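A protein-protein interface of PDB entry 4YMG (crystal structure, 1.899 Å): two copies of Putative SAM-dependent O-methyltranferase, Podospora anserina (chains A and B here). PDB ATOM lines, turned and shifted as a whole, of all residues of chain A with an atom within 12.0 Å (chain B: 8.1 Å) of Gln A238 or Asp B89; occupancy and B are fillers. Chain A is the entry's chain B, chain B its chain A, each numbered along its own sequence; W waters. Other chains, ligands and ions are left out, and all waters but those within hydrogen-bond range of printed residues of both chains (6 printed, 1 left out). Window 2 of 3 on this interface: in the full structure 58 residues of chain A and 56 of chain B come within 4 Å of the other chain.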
ATOM      1  N   ALA A 165      23.439  -3.198  35.512  1.00  0.00           N
ATOM      2  CA  ALA A 165      23.111  -3.925  34.288  1.00  0.00           C
ATOM      3  C   ALA A 165      23.694  -3.278  33.027  1.00  0.00           C
ATOM      4  O   ALA A 165      23.935  -3.967  32.020  1.00  0.00           O
ATOM      5  CB  ALA A 165      21.597  -4.050  34.154  1.00  0.00           C
ATOM      6  N   ASN A 166      23.892  -1.960  33.060  1.00  0.00           N
ATOM      7  CA  ASN A 166      24.469  -1.258  31.898  1.00  0.00           C
ATOM      8  C   ASN A 166      25.933  -0.887  32.085  1.00  0.00           C
ATOM      9  O   ASN A 166      26.489  -0.112  31.297  1.00  0.00           O
ATOM     10  CB  ASN A 166      23.689   0.028  31.586  1.00  0.00           C
ATOM     11  CG  ASN A 166      22.227  -0.227  31.348  1.00  0.00           C
ATOM     12  OD1 ASN A 166      21.843  -1.255  30.785  1.00  0.00           O
ATOM     13  ND2 ASN A 166      21.396   0.719  31.760  1.00  0.00           N
ATOM     14  N   ASP A 218      30.644 -11.298  30.541  1.00  0.00           N
ATOM     15  CA  ASP A 218      31.413 -11.192  29.302  1.00  0.00           C
ATOM     16  C   ASP A 218      32.742 -10.549  29.647  1.00  0.00           C
ATOM     17  O   ASP A 218      32.791  -9.627  30.462  1.00  0.00           O
ATOM     18  CB  ASP A 218      30.695 -10.345  28.253  1.00  0.00           C
ATOM     19  CG  ASP A 218      29.411 -10.975  27.763  1.00  0.00           C
ATOM     20  OD1 ASP A 218      29.389 -12.206  27.546  1.00  0.00           O
ATOM     21  OD2 ASP A 218      28.425 -10.226  27.598  1.00  0.00           O
ATOM     22  N   ARG A 232      31.582  -7.039  31.905  1.00  0.00           N
ATOM     23  CA  ARG A 232      30.190  -6.648  32.023  1.00  0.00           C
ATOM     24  C   ARG A 232      29.389  -7.880  32.384  1.00  0.00           C
ATOM     25  O   ARG A 232      29.830  -9.007  32.117  1.00  0.00           O
ATOM     26  CB  ARG A 232      29.662  -6.026  30.713  1.00  0.00           C
ATOM     27  CG  ARG A 232      29.588  -7.008  29.531  1.00  0.00           C
ATOM     28  CD  ARG A 232      29.136  -6.353  28.228  1.00  0.00           C
ATOM     29  NE  ARG A 232      27.740  -5.927  28.295  1.00  0.00           N
ATOM     30  CZ  ARG A 232      26.711  -6.684  27.932  1.00  0.00           C
ATOM     31  NH1 ARG A 232      26.918  -7.904  27.464  1.00  0.00           N
ATOM     32  NH2 ARG A 232      25.468  -6.224  28.044  1.00  0.00           N
ATOM     33  N   TRP A 233      28.223  -7.678  32.992  1.00  0.00           N
ATOM     34  CA  TRP A 233      27.243  -8.756  33.077  1.00  0.00           C
ATOM     35  C   TRP A 233      26.864  -9.213  31.666  1.00  0.00           C
ATOM     36  O   TRP A 233      26.738  -8.387  30.757  1.00  0.00           O
ATOM     37  CB  TRP A 233      25.971  -8.296  33.796  1.00  0.00           C
ATOM     38  CG  TRP A 233      26.109  -8.000  35.249  1.00  0.00           C
ATOM     39  CD1 TRP A 233      25.951  -6.794  35.851  1.00  0.00           C
ATOM     40  CD2 TRP A 233      26.409  -8.934  36.292  1.00  0.00           C
ATOM     41  NE1 TRP A 233      26.141  -6.909  37.207  1.00  0.00           N
ATOM     42  CE2 TRP A 233      26.414  -8.217  37.506  1.00  0.00           C
ATOM     43  CE3 TRP A 233      26.675 -10.308  36.319  1.00  0.00           C
ATOM     44  CZ2 TRP A 233      26.684  -8.823  38.734  1.00  0.00           C
ATOM     45  CZ3 TRP A 233      26.928 -10.913  37.544  1.00  0.00           C
ATOM     46  CH2 TRP A 233      26.933 -10.168  38.736  1.00  0.00           C
ATOM     47  N   LYS A 234      26.651 -10.511  31.477  1.00  0.00           N
ATOM     48  CA  LYS A 234      26.024 -10.974  30.238  1.00  0.00           C
ATOM     49  C   LYS A 234      24.633 -10.350  30.079  1.00  0.00           C
ATOM     50  O   LYS A 234      24.017  -9.923  31.064  1.00  0.00           O
ATOM     51  CB  LYS A 234      25.918 -12.504  30.216  1.00  0.00           C
ATOM     52  CG  LYS A 234      27.239 -13.207  29.979  1.00  0.00           C
ATOM     53  CD  LYS A 234      27.025 -14.672  29.618  1.00  0.00           C
ATOM     54  CE  LYS A 234      28.352 -15.434  29.548  1.00  0.00           C
ATOM     55  NZ  LYS A 234      29.319 -14.861  28.565  1.00  0.00           N
ATOM     56  N   ASP A 235      24.152 -10.292  28.842  1.00  0.00           N
ATOM     57  CA  ASP A 235      22.812  -9.809  28.535  1.00  0.00           C
ATOM     58  C   ASP A 235      21.771 -10.520  29.386  1.00  0.00           C
ATOM     59  O   ASP A 235      21.867 -11.730  29.586  1.00  0.00           O
ATOM     60  CB  ASP A 235      22.473 -10.045  27.064  1.00  0.00           C
ATOM     61  CG  ASP A 235      23.303  -9.200  26.117  1.00  0.00           C
ATOM     62  OD1 ASP A 235      23.877  -8.182  26.558  1.00  0.00           O
ATOM     63  OD2 ASP A 235      23.364  -9.565  24.923  1.00  0.00           O
ATOM     64  N   GLY A 236      20.776  -9.781  29.871  1.00  0.00           N
ATOM     65  CA  GLY A 236      19.659 -10.404  30.572  1.00  0.00           C
ATOM     66  C   GLY A 236      18.821 -11.310  29.675  1.00  0.00           C
ATOM     67  O   GLY A 236      18.903 -11.254  28.437  1.00  0.00           O
ATOM     68  N   ALA A 237      17.998 -12.142  30.306  1.00  0.00           N
ATOM     69  CA  ALA A 237      17.134 -13.065  29.589  1.00  0.00           C
ATOM     70  C   ALA A 237      16.143 -12.304  28.723  1.00  0.00           C
ATOM     71  O   ALA A 237      15.406 -11.447  29.202  1.00  0.00           O
ATOM     72  CB  ALA A 237      16.401 -13.980  30.565  1.00  0.00           C
ATOM     73  N   GLN A 238      16.136 -12.619  27.439  1.00  0.00           N
ATOM     74  CA  GLN A 238      15.279 -11.920  26.494  1.00  0.00           C
ATOM     75  C   GLN A 238      13.833 -12.443  26.523  1.00  0.00           C
ATOM     76  O   GLN A 238      12.876 -11.686  26.337  1.00  0.00           O
ATOM     77  CB  GLN A 238      15.880 -12.063  25.102  1.00  0.00           C
ATOM     78  CG  GLN A 238      15.488 -11.006  24.118  1.00  0.00           C
ATOM     79  CD  GLN A 238      16.230 -11.169  22.816  1.00  0.00           C
ATOM     80  OE1 GLN A 238      17.183 -11.951  22.725  1.00  0.00           O
ATOM     81  NE2 GLN A 238      15.794 -10.452  21.792  1.00  0.00           N
ATOM     82  N   ARG A 239      13.680 -13.746  26.761  1.00  0.00           N
ATOM     83  CA  ARG A 239      12.365 -14.394  26.694  1.00  0.00           C
ATOM     84  C   ARG A 239      12.076 -15.226  27.949  1.00  0.00           C
ATOM     85  O   ARG A 239      12.988 -15.769  28.563  1.00  0.00           O
ATOM     86  CB  ARG A 239      12.284 -15.279  25.446  1.00  0.00           C
ATOM     87  CG  ARG A 239      12.534 -14.523  24.136  1.00  0.00           C
ATOM     88  CD  ARG A 239      12.480 -15.446  22.926  1.00  0.00           C
ATOM     89  NE  ARG A 239      12.479 -14.701  21.669  1.00  0.00           N
ATOM     90  CZ  ARG A 239      13.573 -14.327  21.012  1.00  0.00           C
ATOM     91  NH1 ARG A 239      14.776 -14.625  21.492  1.00  0.00           N
ATOM     92  NH2 ARG A 239      13.468 -13.656  19.871  1.00  0.00           N
ATOM     93  N   ALA A 240      10.804 -15.336  28.317  1.00  0.00           N
ATOM     94  CA  ALA A 240      10.423 -16.082  29.514  1.00  0.00           C
ATOM     95  C   ALA A 240      10.533 -17.603  29.310  1.00  0.00           C
ATOM     96  O   ALA A 240      10.499 -18.083  28.174  1.00  0.00           O
ATOM     97  CB  ALA A 240       9.003 -15.701  29.933  1.00  0.00           C
ATOM     98  N   ALA B  61      30.019  -4.010  20.829  1.00  0.00           N
ATOM     99  CA  ALA B  61      28.613  -4.001  20.429  1.00  0.00           C
ATOM    100  C   ALA B  61      27.688  -4.508  21.538  1.00  0.00           C
ATOM    101  O   ALA B  61      26.608  -3.958  21.737  1.00  0.00           O
ATOM    102  CB  ALA B  61      28.410  -4.833  19.154  1.00  0.00           C
ATOM    103  N   ARG B  62      28.085  -5.566  22.247  1.00  0.00           N
ATOM    104  CA  ARG B  62      27.229  -6.079  23.334  1.00  0.00           C
ATOM    105  C   ARG B  62      27.102  -5.047  24.435  1.00  0.00           C
ATOM    106  O   ARG B  62      26.038  -4.869  25.023  1.00  0.00           O
ATOM    107  CB  ARG B  62      27.780  -7.372  23.939  1.00  0.00           C
ATOM    108  CG  ARG B  62      27.655  -8.564  23.038  1.00  0.00           C
ATOM    109  CD  ARG B  62      28.101  -9.854  23.728  1.00  0.00           C
ATOM    110  NE  ARG B  62      28.080 -10.930  22.745  1.00  0.00           N
ATOM    111  CZ  ARG B  62      28.091 -12.225  23.024  1.00  0.00           C
ATOM    112  NH1 ARG B  62      28.131 -12.635  24.284  1.00  0.00           N
ATOM    113  NH2 ARG B  62      28.061 -13.106  22.034  1.00  0.00           N
ATOM    114  N   ASP B  63      28.213  -4.380  24.712  1.00  0.00           N
ATOM    115  CA  ASP B  63      28.285  -3.357  25.748  1.00  0.00           C
ATOM    116  C   ASP B  63      27.427  -2.136  25.394  1.00  0.00           C
ATOM    117  O   ASP B  63      26.470  -1.800  26.098  1.00  0.00           O
ATOM    118  CB  ASP B  63      29.750  -2.956  25.939  1.00  0.00           C
ATOM    119  CG  ASP B  63      29.939  -1.822  26.926  1.00  0.00           C
ATOM    120  OD1 ASP B  63      29.184  -1.745  27.910  1.00  0.00           O
ATOM    121  OD2 ASP B  63      30.879  -1.025  26.727  1.00  0.00           O
ATOM    122  N   ARG B  64      27.792  -1.474  24.300  1.00  0.00           N
ATOM    123  CA  ARG B  64      27.178  -0.204  23.922  1.00  0.00           C
ATOM    124  C   ARG B  64      25.762  -0.369  23.379  1.00  0.00           C
ATOM    125  O   ARG B  64      24.984   0.571  23.419  1.00  0.00           O
ATOM    126  CB  ARG B  64      28.032   0.509  22.870  1.00  0.00           C
ATOM    127  CG  ARG B  64      29.487   0.734  23.271  1.00  0.00           C
ATOM    128  CD  ARG B  64      30.208   1.509  22.158  1.00  0.00           C
ATOM    129  NE  ARG B  64      29.598   2.827  21.995  1.00  0.00           N
ATOM    130  CZ  ARG B  64      30.032   3.919  22.616  1.00  0.00           C
ATOM    131  NH1 ARG B  64      31.091   3.850  23.414  1.00  0.00           N
ATOM    132  NH2 ARG B  64      29.423   5.085  22.423  1.00  0.00           N
ATOM    133  N   LYS B  65      25.458  -1.554  22.847  1.00  0.00           N
ATOM    134  CA  LYS B  65      24.179  -1.827  22.180  1.00  0.00           C
ATOM    135  C   LYS B  65      23.762  -0.730  21.173  1.00  0.00           C
ATOM    136  O   LYS B  65      22.693  -0.130  21.295  1.00  0.00           O
ATOM    137  CB  LYS B  65      23.083  -2.037  23.235  1.00  0.00           C
ATOM    138  CG  LYS B  65      23.454  -3.122  24.251  1.00  0.00           C
ATOM    139  CD  LYS B  65      22.232  -3.843  24.842  1.00  0.00           C
ATOM    140  CE  LYS B  65      22.665  -4.998  25.751  1.00  0.00           C
ATOM    141  NZ  LYS B  65      23.555  -6.007  25.054  1.00  0.00           N
ATOM    142  N   PRO B  66      24.610  -0.469  20.170  1.00  0.00           N
ATOM    143  CA  PRO B  66      24.212   0.484  19.129  1.00  0.00           C
ATOM    144  C   PRO B  66      23.031  -0.056  18.318  1.00  0.00           C
ATOM    145  O   PRO B  66      22.937  -1.260  18.100  1.00  0.00           O
ATOM    146  CB  PRO B  66      25.477   0.615  18.269  1.00  0.00           C
ATOM    147  CG  PRO B  66      26.215  -0.668  18.484  1.00  0.00           C
ATOM    148  CD  PRO B  66      25.927  -1.082  19.897  1.00  0.00           C
ATOM    149  N   TRP B  83      29.956  -7.405  14.211  1.00  0.00           N
ATOM    150  CA  TRP B  83      28.925  -6.460  14.641  1.00  0.00           C
ATOM    151  C   TRP B  83      27.571  -7.163  14.719  1.00  0.00           C
ATOM    152  O   TRP B  83      26.807  -6.973  15.672  1.00  0.00           O
ATOM    153  CB  TRP B  83      28.831  -5.242  13.691  1.00  0.00           C
ATOM    154  CG  TRP B  83      30.101  -4.453  13.537  1.00  0.00           C
ATOM    155  CD1 TRP B  83      30.710  -4.112  12.362  1.00  0.00           C
ATOM    156  CD2 TRP B  83      30.922  -3.915  14.584  1.00  0.00           C
ATOM    157  NE1 TRP B  83      31.860  -3.400  12.610  1.00  0.00           N
ATOM    158  CE2 TRP B  83      32.011  -3.260  13.965  1.00  0.00           C
ATOM    159  CE3 TRP B  83      30.832  -3.901  15.981  1.00  0.00           C
ATOM    160  CZ2 TRP B  83      33.009  -2.609  14.696  1.00  0.00           C
ATOM    161  CZ3 TRP B  83      31.835  -3.249  16.714  1.00  0.00           C
ATOM    162  CH2 TRP B  83      32.904  -2.612  16.063  1.00  0.00           C
ATOM    163  N   TYR B  84      27.295  -7.995  13.717  1.00  0.00           N
ATOM    164  CA  TYR B  84      26.068  -8.809  13.668  1.00  0.00           C
ATOM    165  C   TYR B  84      25.905  -9.683  14.914  1.00  0.00           C
ATOM    166  O   TYR B  84      24.822  -9.743  15.523  1.00  0.00           O
ATOM    167  CB  TYR B  84      26.079  -9.681  12.400  1.00  0.00           C
ATOM    168  CG  TYR B  84      24.940 -10.689  12.289  1.00  0.00           C
ATOM    169  CD1 TYR B  84      23.711 -10.326  11.744  1.00  0.00           C
ATOM    170  CD2 TYR B  84      25.107 -12.012  12.706  1.00  0.00           C
ATOM    171  CE1 TYR B  84      22.669 -11.250  11.632  1.00  0.00           C
ATOM    172  CE2 TYR B  84      24.069 -12.944  12.596  1.00  0.00           C
ATOM    173  CZ  TYR B  84      22.859 -12.555  12.062  1.00  0.00           C
ATOM    174  OH  TYR B  84      21.841 -13.476  11.947  1.00  0.00           O
ATOM    175  N   GLU B  85      26.990 -10.350  15.293  1.00  0.00           N
ATOM    176  CA  GLU B  85      26.971 -11.271  16.424  1.00  0.00           C
ATOM    177  C   GLU B  85      26.769 -10.527  17.738  1.00  0.00           C
ATOM    178  O   GLU B  85      26.129 -11.042  18.646  1.00  0.00           O
ATOM    179  CB  GLU B  85      28.272 -12.086  16.479  1.00  0.00           C
ATOM    180  CG  GLU B  85      28.349 -13.230  15.458  1.00  0.00           C
ATOM    181  CD  GLU B  85      27.447 -14.400  15.828  1.00  0.00           C
ATOM    182  OE1 GLU B  85      26.885 -14.399  16.946  1.00  0.00           O
ATOM    183  OE2 GLU B  85      27.311 -15.320  15.005  1.00  0.00           O
ATOM    184  N   GLY B  86      27.319  -9.318  17.831  1.00  0.00           N
ATOM    185  CA  GLY B  86      27.215  -8.534  19.051  1.00  0.00           C
ATOM    186  C   GLY B  86      25.914  -7.765  19.177  1.00  0.00           C
ATOM    187  O   GLY B  86      25.698  -7.060  20.167  1.00  0.00           O
ATOM    188  N   THR B  87      25.047  -7.904  18.176  1.00  0.00           N
ATOM    189  CA  THR B  87      23.787  -7.170  18.140  1.00  0.00           C
ATOM    190  C   THR B  87      22.603  -8.089  17.830  1.00  0.00           C
ATOM    191  O   THR B  87      21.574  -7.640  17.326  1.00  0.00           O
ATOM    192  CB  THR B  87      23.826  -6.020  17.090  1.00  0.00           C
ATOM    193  OG1 THR B  87      24.072  -6.553  15.774  1.00  0.00           O
ATOM    194  CG2 THR B  87      24.902  -4.988  17.441  1.00  0.00           C
ATOM    195  N   ARG B  88      22.749  -9.377  18.131  1.00  0.00           N
ATOM    196  CA  ARG B  88      21.648 -10.323  17.958  1.00  0.00           C
ATOM    197  C   ARG B  88      20.470  -9.980  18.864  1.00  0.00           C
ATOM    198  O   ARG B  88      19.333 -10.283  18.537  1.00  0.00           O
ATOM    199  CB  ARG B  88      22.099 -11.752  18.242  1.00  0.00           C
ATOM    200  CG  ARG B  88      22.925 -12.407  17.146  1.00  0.00           C
ATOM    201  CD  ARG B  88      23.153 -13.865  17.516  1.00  0.00           C
ATOM    202  NE  ARG B  88      24.017 -14.572  16.577  1.00  0.00           N
ATOM    203  CZ  ARG B  88      23.566 -15.247  15.526  1.00  0.00           C
ATOM    204  NH1 ARG B  88      22.264 -15.277  15.277  1.00  0.00           N
ATOM    205  NH2 ARG B  88      24.413 -15.879  14.718  1.00  0.00           N
ATOM    206  N   ASP B  89      20.740  -9.344  19.999  1.00  0.00           N
ATOM    207  CA  ASP B  89      19.669  -9.038  20.944  1.00  0.00           C
ATOM    208  C   ASP B  89      18.830  -7.846  20.482  1.00  0.00           C
ATOM    209  O   ASP B  89      17.631  -7.783  20.745  1.00  0.00           O
ATOM    210  CB  ASP B  89      20.233  -8.784  22.350  1.00  0.00           C
ATOM    211  CG  ASP B  89      21.239  -7.624  22.399  1.00  0.00           C
ATOM    212  OD1 ASP B  89      21.986  -7.401  21.410  1.00  0.00           O
ATOM    213  OD2 ASP B  89      21.286  -6.943  23.450  1.00  0.00           O
ATOM    214  N   THR B  90      19.459  -6.912  19.784  1.00  0.00           N
ATOM    215  CA  THR B  90      18.781  -5.698  19.342  1.00  0.00           C
ATOM    216  C   THR B  90      18.364  -5.772  17.874  1.00  0.00           C
ATOM    217  O   THR B  90      17.545  -4.975  17.417  1.00  0.00           O
ATOM    218  CB  THR B  90      19.678  -4.464  19.526  1.00  0.00           C
ATOM    219  OG1 THR B  90      20.866  -4.622  18.738  1.00  0.00           O
ATOM    220  CG2 THR B  90      20.054  -4.282  20.989  1.00  0.00           C
ATOM    221  N   LYS B  91      18.940  -6.730  17.149  1.00  0.00           N
ATOM    222  CA  LYS B  91      18.773  -6.831  15.693  1.00  0.00           C
ATOM    223  C   LYS B  91      19.145  -5.499  15.039  1.00  0.00           C
ATOM    224  O   LYS B  91      18.467  -5.026  14.133  1.00  0.00           O
ATOM    225  CB  LYS B  91      17.335  -7.238  15.316  1.00  0.00           C
ATOM    226  CG  LYS B  91      16.886  -8.586  15.884  1.00  0.00           C
ATOM    227  CD  LYS B  91      17.858  -9.695  15.514  1.00  0.00           C
ATOM    228  CE  LYS B  91      17.465 -11.036  16.132  1.00  0.00           C
ATOM    229  NZ  LYS B  91      18.595 -12.023  16.110  1.00  0.00           N
ATOM    230  N   ALA B  92      20.236  -4.899  15.504  1.00  0.00           N
ATOM    231  CA  ALA B  92      20.721  -3.645  14.938  1.00  0.00           C
ATOM    232  C   ALA B  92      20.928  -3.747  13.426  1.00  0.00           C
ATOM    233  O   ALA B  92      21.394  -4.772  12.917  1.00  0.00           O
ATOM    234  CB  ALA B  92      22.022  -3.235  15.611  1.00  0.00           C
ATOM    235  N   ARG B 119      18.988  -7.226   7.782  1.00  0.00           N
ATOM    236  CA  ARG B 119      19.495  -6.153   8.641  1.00  0.00           C
ATOM    237  C   ARG B 119      20.980  -5.891   8.376  1.00  0.00           C
ATOM    238  O   ARG B 119      21.519  -4.869   8.794  1.00  0.00           O
ATOM    239  CB  ARG B 119      19.258  -6.460  10.126  1.00  0.00           C
ATOM    240  CG  ARG B 119      20.179  -7.488  10.775  1.00  0.00           C
ATOM    241  CD  ARG B 119      19.825  -7.579  12.262  1.00  0.00           C
ATOM    242  NE  ARG B 119      20.482  -8.665  12.988  1.00  0.00           N
ATOM    243  CZ  ARG B 119      21.564  -8.505  13.749  1.00  0.00           C
ATOM    244  NH1 ARG B 119      22.132  -7.307  13.847  1.00  0.00           N
ATOM    245  NH2 ARG B 119      22.093  -9.542  14.394  1.00  0.00           N
HETATM  246  O   HOH W   1      16.875 -10.928  19.364  1.00  0.00           O
HETATM  247  O   HOH W   2      16.604 -13.807  18.350  1.00  0.00           O
HETATM  248  O   HOH W   3      27.634 -14.248  26.292  1.00  0.00           O
HETATM  249  O   HOH W   4      27.710  -3.285  29.530  1.00  0.00           O
HETATM  250  O   HOH W   5      14.948  -7.410  20.522  1.00  0.00           O
HETATM  251  O   HOH W   6      25.448  -3.082  28.270  1.00  0.00           O
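Among the printed residues, merely in contact across the chains: Arg A232 with Asp B63, Arg A232 with Lys B65 and Asp A235 with Asp B89.
No position is printed for both chains.
Of the 12 printed residues of chain A, 4 touch a printed residue of chain B. Along chain A the printed residues that touch a printed residue of chain B span positions 218 to 238. Among the printed residues, Asp or Glu carboxylates within 4 Å of a Lys or Arg side-chain nitrogen of the other chain: Asp A218 with Arg B62 (3.5 Å) and Asp A235 with Lys B65 (2.7 Å).
O of Arg B62 lies within hydrogen-bond range of NZ of Lys B65, at 2.7 Å. The side-chain carboxylate (OD2) of Asp B89 is in salt-bridge range of the side-chain amino group (NZ) of Lys B65, at 2.9 Å. The side-chain carboxylate (OD2) of Asp A218 lies within salt-bridge range of the guanidinium group (NH1) of Arg A232 (2.8 Å). The side-chain carboxylate (OD1) of Asp A218 lies within salt-bridge range of the side-chain amino group (NZ) of Lys A234, 2.8 Å away. The side-chain carboxylate of Asp A235 is in salt-bridge range of the guanidinium group of Arg A232 (2.9 Å).
The side-chain amide nitrogen (NE2) of Gln A238 is in hydrogen-bond range of the backbone carbonyl oxygen (O) of Asp B89. O of Arg B62 sits at hydrogen-bond distance from NH2 of Arg A232 (3.4 Å). The side-chain amino group (NZ) of Lys B65 lies within salt-bridge range of the side-chain carboxylate (OD1) of Asp A235, at 2.7 Å. NH1 of Arg B62 is in salt-bridge range of OD1 of Asp A218 (3.5 Å).
Gln A238 touches just one residue of chain B: Asp B89 (3.4 Å). Asp B89 touches just these residues of chain A: Asp A235 and Gln A238. Thr B87 touches none of the printed residues of chain A. No residue of chain A comes within 4 Å of Thr B90. Of the printed residues of chain A, Arg B62 touches Asp A218 (3.5 Å) and Arg A232 (3.4 Å). Printed residues of chain B within 4 Å of Asp A218: Arg B62 (3.5 Å). Of the printed residues of chain B, Asp A235 touches Lys B65 and Asp B89. Printed residues of chain A within 4 Å of Asp B63: Arg A232 (3.7 Å). Pro B66 touches none of the printed residues of chain A. The nearest residue of chain A that does not touch Asp B89 is Arg A232 (6.3 Å). The nearest printed residue of chain B that does not touch Arg A232 is Arg B64 (6.0 Å).
Water W3 lies within hydrogen-bond range of the guanidinium group (NH1) of Arg B62 (2.6 Å), the side-chain amino group (NZ) of Lys A234 (2.9 Å) and the side-chain carboxylate (OD1) of Asp A218 (3.0 Å). Water W1 lies within hydrogen-bond range of the backbone carbonyl oxygen of Arg B88 (2.7 Å) and the side-chain amide nitrogen of Gln A238 (2.7 Å). Water W4 bridges the side-chain carboxylate (OD1) of Asp B63 (2.7 Å) and the guanidinium group (NE) of Arg A232 (2.9 Å). Water W5 bridges the backbone carbonyl oxygen of Asp B89 (2.7 Å) and the side-chain amide nitrogen of Gln A238 (3.4 Å). Water W6 lies within hydrogen-bond range of O of Asp B63 and NH2 of Arg A232. Water W2 bridges the guanidinium group of Arg A239 and the side-chain amino group of Lys B91.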
